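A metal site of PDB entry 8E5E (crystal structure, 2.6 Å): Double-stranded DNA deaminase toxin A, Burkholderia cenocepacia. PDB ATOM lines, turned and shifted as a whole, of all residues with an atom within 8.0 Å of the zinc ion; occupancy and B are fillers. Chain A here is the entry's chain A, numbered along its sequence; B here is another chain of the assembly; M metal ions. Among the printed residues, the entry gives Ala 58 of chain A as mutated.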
ATOM      1  N   THR A  22       7.456  35.474 -22.621  1.00  0.00           N
ATOM      2  CA  THR A  22       6.967  34.309 -21.892  1.00  0.00           C
ATOM      3  C   THR A  22       8.143  33.515 -21.332  1.00  0.00           C
ATOM      4  O   THR A  22       8.980  33.014 -22.100  1.00  0.00           O
ATOM      5  CB  THR A  22       6.099  33.438 -22.789  1.00  0.00           C
ATOM      6  OG1 THR A  22       5.038  34.224 -23.348  1.00  0.00           O
ATOM      7  CG2 THR A  22       5.499  32.283 -22.002  1.00  0.00           C
ATOM      8  N   ALA A  52       6.279  28.343 -36.463  1.00  0.00           N
ATOM      9  CA  ALA A  52       5.918  29.522 -35.676  1.00  0.00           C
ATOM     10  C   ALA A  52       5.977  29.276 -34.177  1.00  0.00           C
ATOM     11  O   ALA A  52       6.009  30.231 -33.404  1.00  0.00           O
ATOM     12  CB  ALA A  52       4.521  30.013 -36.063  1.00  0.00           C
ATOM     13  N   ASN A  53       6.002  28.011 -33.745  1.00  0.00           N
ATOM     14  CA  ASN A  53       6.025  27.662 -32.339  1.00  0.00           C
ATOM     15  C   ASN A  53       7.419  27.344 -31.828  1.00  0.00           C
ATOM     16  O   ASN A  53       7.583  27.093 -30.628  1.00  0.00           O
ATOM     17  CB  ASN A  53       5.096  26.476 -32.072  1.00  0.00           C
ATOM     18  CG  ASN A  53       5.474  25.251 -32.876  1.00  0.00           C
ATOM     19  OD1 ASN A  53       6.066  25.352 -33.951  1.00  0.00           O
ATOM     20  ND2 ASN A  53       5.151  24.076 -32.348  1.00  0.00           N
ATOM     21  N   ALA A  54       8.431  27.350 -32.693  1.00  0.00           N
ATOM     22  CA  ALA A  54       9.773  26.984 -32.277  1.00  0.00           C
ATOM     23  C   ALA A  54      10.388  28.018 -31.328  1.00  0.00           C
ATOM     24  O   ALA A  54      11.239  27.669 -30.503  1.00  0.00           O
ATOM     25  CB  ALA A  54      10.671  26.794 -33.492  1.00  0.00           C
ATOM     26  N   GLY A  55       9.976  29.271 -31.433  1.00  0.00           N
ATOM     27  CA  GLY A  55      10.472  30.302 -30.549  1.00  0.00           C
ATOM     28  C   GLY A  55       9.754  30.408 -29.219  1.00  0.00           C
ATOM     29  O   GLY A  55      10.124  31.238 -28.387  1.00  0.00           O
ATOM     30  N   HIS A  56       8.741  29.584 -29.003  1.00  0.00           N
ATOM     31  CA  HIS A  56       7.942  29.626 -27.786  1.00  0.00           C
ATOM     32  C   HIS A  56       8.505  28.681 -26.735  1.00  0.00           C
ATOM     33  O   HIS A  56       9.384  27.861 -27.007  1.00  0.00           O
ATOM     34  CB  HIS A  56       6.485  29.265 -28.098  1.00  0.00           C
ATOM     35  CG  HIS A  56       5.830  30.178 -29.093  1.00  0.00           C
ATOM     36  ND1 HIS A  56       4.487  30.088 -29.405  1.00  0.00           N
ATOM     37  CD2 HIS A  56       6.335  31.182 -29.847  1.00  0.00           C
ATOM     38  CE1 HIS A  56       4.199  31.007 -30.313  1.00  0.00           C
ATOM     39  NE2 HIS A  56       5.296  31.681 -30.598  1.00  0.00           N
ATOM     40  N   VAL A  57       7.976  28.790 -25.518  1.00  0.00           N
ATOM     41  CA  VAL A  57       8.465  27.964 -24.416  1.00  0.00           C
ATOM     42  C   VAL A  57       8.144  26.493 -24.674  1.00  0.00           C
ATOM     43  O   VAL A  57       8.975  25.616 -24.444  1.00  0.00           O
ATOM     44  CB  VAL A  57       7.890  28.449 -23.082  1.00  0.00           C
ATOM     45  CG1 VAL A  57       8.404  27.601 -21.937  1.00  0.00           C
ATOM     46  CG2 VAL A  57       8.235  29.920 -22.861  1.00  0.00           C
ATOM     47  N   ALA A  58       6.925  26.207 -25.153  1.00  0.00           N
ATOM     48  CA  ALA A  58       6.549  24.830 -25.434  1.00  0.00           C
ATOM     49  C   ALA A  58       7.383  24.247 -26.573  1.00  0.00           C
ATOM     50  O   ALA A  58       7.784  23.083 -26.532  1.00  0.00           O
ATOM     51  CB  ALA A  58       5.057  24.737 -25.750  1.00  0.00           C
ATOM     52  N   GLY A  59       7.650  25.049 -27.605  1.00  0.00           N
ATOM     53  CA  GLY A  59       8.454  24.572 -28.716  1.00  0.00           C
ATOM     54  C   GLY A  59       9.894  24.333 -28.335  1.00  0.00           C
ATOM     55  O   GLY A  59      10.501  23.331 -28.721  1.00  0.00           O
ATOM     56  N   HIS A  77       4.351  27.828 -17.797  1.00  0.00           N
ATOM     57  CA  HIS A  77       4.681  29.158 -18.282  1.00  0.00           C
ATOM     58  C   HIS A  77       3.784  30.197 -17.615  1.00  0.00           C
ATOM     59  O   HIS A  77       2.908  29.870 -16.805  1.00  0.00           O
ATOM     60  CB  HIS A  77       4.583  29.243 -19.814  1.00  0.00           C
ATOM     61  CG  HIS A  77       3.194  29.117 -20.352  1.00  0.00           C
ATOM     62  ND1 HIS A  77       2.297  30.171 -20.359  1.00  0.00           N
ATOM     63  CD2 HIS A  77       2.550  28.074 -20.921  1.00  0.00           C
ATOM     64  CE1 HIS A  77       1.161  29.773 -20.908  1.00  0.00           C
ATOM     65  NE2 HIS A  77       1.283  28.501 -21.261  1.00  0.00           N
ATOM     66  N   ASN A  79       2.372  33.078 -19.438  1.00  0.00           N
ATOM     67  CA  ASN A  79       1.639  33.904 -20.398  1.00  0.00           C
ATOM     68  C   ASN A  79       0.152  33.889 -20.078  1.00  0.00           C
ATOM     69  O   ASN A  79      -0.469  32.819 -20.097  1.00  0.00           O
ATOM     70  CB  ASN A  79       1.891  33.421 -21.817  1.00  0.00           C
ATOM     71  CG  ASN A  79       1.188  34.269 -22.858  1.00  0.00           C
ATOM     72  OD1 ASN A  79       0.017  34.059 -23.157  1.00  0.00           O
ATOM     73  ND2 ASN A  79       1.908  35.219 -23.424  1.00  0.00           N
ATOM     74  N   GLY A  82      -2.641  32.311 -22.596  1.00  0.00           N
ATOM     75  CA  GLY A  82      -2.717  30.885 -22.842  1.00  0.00           C
ATOM     76  C   GLY A  82      -1.640  30.389 -23.783  1.00  0.00           C
ATOM     77  O   GLY A  82      -0.624  31.047 -24.026  1.00  0.00           O
ATOM     78  N   THR A  83      -1.874  29.199 -24.322  1.00  0.00           N
ATOM     79  CA  THR A  83      -0.960  28.552 -25.249  1.00  0.00           C
ATOM     80  C   THR A  83      -1.459  28.788 -26.670  1.00  0.00           C
ATOM     81  O   THR A  83      -2.610  28.470 -26.986  1.00  0.00           O
ATOM     82  CB  THR A  83      -0.856  27.052 -24.946  1.00  0.00           C
ATOM     83  OG1 THR A  83      -0.381  26.871 -23.607  1.00  0.00           O
ATOM     84  CG2 THR A  83       0.094  26.383 -25.922  1.00  0.00           C
ATOM     85  N   CYS A  84      -0.588  29.335 -27.525  1.00  0.00           N
ATOM     86  CA  CYS A  84      -0.993  29.711 -28.870  1.00  0.00           C
ATOM     87  C   CYS A  84      -1.436  28.496 -29.678  1.00  0.00           C
ATOM     88  O   CYS A  84      -1.073  27.348 -29.382  1.00  0.00           O
ATOM     89  CB  CYS A  84       0.148  30.418 -29.589  1.00  0.00           C
ATOM     90  SG  CYS A  84       1.487  29.331 -30.102  1.00  0.00           S
ATOM     91  N   GLY A  85      -2.230  28.753 -30.722  1.00  0.00           N
ATOM     92  CA  GLY A  85      -2.711  27.670 -31.568  1.00  0.00           C
ATOM     93  C   GLY A  85      -1.620  26.991 -32.361  1.00  0.00           C
ATOM     94  O   GLY A  85      -1.733  25.798 -32.677  1.00  0.00           O
ATOM     95  N   PHE A  86      -0.562  27.723 -32.703  1.00  0.00           N
ATOM     96  CA  PHE A  86       0.615  27.093 -33.298  1.00  0.00           C
ATOM     97  C   PHE A  86       1.136  25.983 -32.399  1.00  0.00           C
ATOM     98  O   PHE A  86       1.053  24.802 -32.733  1.00  0.00           O
ATOM     99  CB  PHE A  86       1.696  28.142 -33.573  1.00  0.00           C
ATOM    100  CG  PHE A  86       1.254  29.246 -34.492  1.00  0.00           C
ATOM    101  CD1 PHE A  86       1.013  28.989 -35.832  1.00  0.00           C
ATOM    102  CD2 PHE A  86       1.098  30.542 -34.031  1.00  0.00           C
ATOM    103  CE1 PHE A  86       0.611  29.992 -36.685  1.00  0.00           C
ATOM    104  CE2 PHE A  86       0.700  31.554 -34.879  1.00  0.00           C
ATOM    105  CZ  PHE A  86       0.456  31.279 -36.206  1.00  0.00           C
ATOM    106  N   CYS A  87       1.581  26.356 -31.188  1.00  0.00           N
ATOM    107  CA  CYS A  87       2.034  25.372 -30.211  1.00  0.00           C
ATOM    108  C   CYS A  87       1.030  24.249 -29.984  1.00  0.00           C
ATOM    109  O   CYS A  87       1.413  23.157 -29.564  1.00  0.00           O
ATOM    110  CB  CYS A  87       2.346  26.064 -28.877  1.00  0.00           C
ATOM    111  SG  CYS A  87       3.838  27.064 -28.890  1.00  0.00           S
ATOM    112  N   VAL A  88      -0.255  24.485 -30.271  1.00  0.00           N
ATOM    113  CA  VAL A  88      -1.259  23.433 -30.130  1.00  0.00           C
ATOM    114  C   VAL A  88      -1.188  22.454 -31.295  1.00  0.00           C
ATOM    115  O   VAL A  88      -1.305  21.238 -31.092  1.00  0.00           O
ATOM    116  CB  VAL A  88      -2.661  24.058 -29.999  1.00  0.00           C
ATOM    117  CG1 VAL A  88      -3.736  22.998 -30.138  1.00  0.00           C
ATOM    118  CG2 VAL A  88      -2.805  24.775 -28.660  1.00  0.00           C
ATOM    119  N   THR A  91       3.273  21.120 -31.944  1.00  0.00           N
ATOM    120  CA  THR A  91       4.145  20.565 -30.915  1.00  0.00           C
ATOM    121  C   THR A  91       4.376  19.073 -31.124  1.00  0.00           C
ATOM    122  O   THR A  91       5.512  18.588 -31.088  1.00  0.00           O
ATOM    123  CB  THR A  91       3.555  20.829 -29.523  1.00  0.00           C
ATOM    124  OG1 THR A  91       3.588  22.233 -29.253  1.00  0.00           O
ATOM    125  CG2 THR A  91       4.342  20.077 -28.453  1.00  0.00           C
ATOM    126  N   VAL A 103       1.741  20.848 -21.069  1.00  0.00           N
ATOM    127  CA  VAL A 103       2.003  22.276 -20.995  1.00  0.00           C
ATOM    128  C   VAL A 103       0.926  22.908 -20.126  1.00  0.00           C
ATOM    129  O   VAL A 103      -0.262  22.874 -20.471  1.00  0.00           O
ATOM    130  CB  VAL A 103       2.026  22.918 -22.395  1.00  0.00           C
ATOM    131  CG1 VAL A 103       2.271  24.415 -22.280  1.00  0.00           C
ATOM    132  CG2 VAL A 103       3.085  22.254 -23.259  1.00  0.00           C
ATOM    133  P    DT B   7      -1.161  35.344 -32.870  1.00  0.00           P
ATOM    134  OP1  DT B   7      -2.052  36.497 -32.670  1.00  0.00           O
ATOM    135  OP2  DT B   7      -0.332  35.256 -34.092  1.00  0.00           O
ATOM    136  O5'  DT B   7      -0.197  35.233 -31.599  1.00  0.00           O
ATOM    137  C5'  DT B   7       0.438  34.000 -31.311  1.00  0.00           C
ATOM    138  C4'  DT B   7       1.891  34.226 -30.950  1.00  0.00           C
ATOM    139  O4'  DT B   7       2.733  33.619 -31.965  1.00  0.00           O
ATOM    140  C3'  DT B   7       2.312  35.704 -30.879  1.00  0.00           C
ATOM    141  O3'  DT B   7       2.954  35.964 -29.641  1.00  0.00           O
ATOM    142  C2'  DT B   7       3.249  35.883 -32.068  1.00  0.00           C
ATOM    143  C1'  DT B   7       3.806  34.480 -32.243  1.00  0.00           C
ATOM    144  N1   DT B   7       4.295  34.187 -33.623  1.00  0.00           N
ATOM    145  C2   DT B   7       5.573  33.731 -33.800  1.00  0.00           C
ATOM    146  O2   DT B   7       6.348  33.538 -32.879  1.00  0.00           O
ATOM    147  N3   DT B   7       5.927  33.508 -35.107  1.00  0.00           N
ATOM    148  C4   DT B   7       5.139  33.683 -36.223  1.00  0.00           C
ATOM    149  O4   DT B   7       5.547  33.455 -37.364  1.00  0.00           O
ATOM    150  C5   DT B   7       3.800  34.167 -35.969  1.00  0.00           C
ATOM    151  C7   DT B   7       2.856  34.411 -37.105  1.00  0.00           C
ATOM    152  C6   DT B   7       3.451  34.394 -34.694  1.00  0.00           C
ATOM    153  P    DC B   8       2.520  37.225 -28.756  1.00  0.00           P
ATOM    154  OP1  DC B   8       1.287  36.847 -28.025  1.00  0.00           O
ATOM    155  OP2  DC B   8       2.521  38.413 -29.628  1.00  0.00           O
ATOM    156  O5'  DC B   8       3.711  37.389 -27.698  1.00  0.00           O
ATOM    157  C5'  DC B   8       3.931  36.394 -26.714  1.00  0.00           C
ATOM    158  C4'  DC B   8       5.412  36.114 -26.545  1.00  0.00           C
ATOM    159  O4'  DC B   8       5.585  34.857 -25.861  1.00  0.00           O
ATOM    160  C3'  DC B   8       6.179  35.970 -27.842  1.00  0.00           C
ATOM    161  O3'  DC B   8       7.560  36.248 -27.632  1.00  0.00           O
ATOM    162  C2'  DC B   8       5.955  34.494 -28.178  1.00  0.00           C
ATOM    163  C1'  DC B   8       5.894  33.839 -26.795  1.00  0.00           C
ATOM    164  N1   DC B   8       4.864  32.769 -26.709  1.00  0.00           N
ATOM    165  C2   DC B   8       5.149  31.579 -26.027  1.00  0.00           C
ATOM    166  O2   DC B   8       6.267  31.441 -25.500  1.00  0.00           O
ATOM    167  N3   DC B   8       4.203  30.612 -25.968  1.00  0.00           N
ATOM    168  C4   DC B   8       3.015  30.808 -26.551  1.00  0.00           C
ATOM    169  N4   DC B   8       2.105  29.835 -26.462  1.00  0.00           N
ATOM    170  C5   DC B   8       2.709  32.012 -27.246  1.00  0.00           C
ATOM    171  C6   DC B   8       3.650  32.953 -27.297  1.00  0.00           C
HETATM  172 ZN    ZN M   1       2.946  29.050 -28.623  1.00  0.00          ZN
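The zinc ion is bound by a ring nitrogen (ND1) of His 56, the side-chain sulfur of Cys 84, the side-chain sulfur of Cys 87 and N4 of DC 8 of chain B.
O2 of DT 7 of chain B lies within hydrogen-bond range of a ring nitrogen (NE2) of His 56 (3.1 Å).
NE2 of His 56 sits at hydrogen-bond distance from O of Ala 52, at 3.2 Å.
The side-chain sulfur (SG) of Cys 84 sits close to the backbone NH (N) of Phe 86 (3.7 Å).
The backbone NH of Val 57 lies within hydrogen-bond range of O2 of DC 8 of chain B, at 3.2 Å.
The side-chain hydroxyl (OG1) of Thr 22 lies within hydrogen-bond range of O4' of DC 8 of chain B (2.6 Å).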
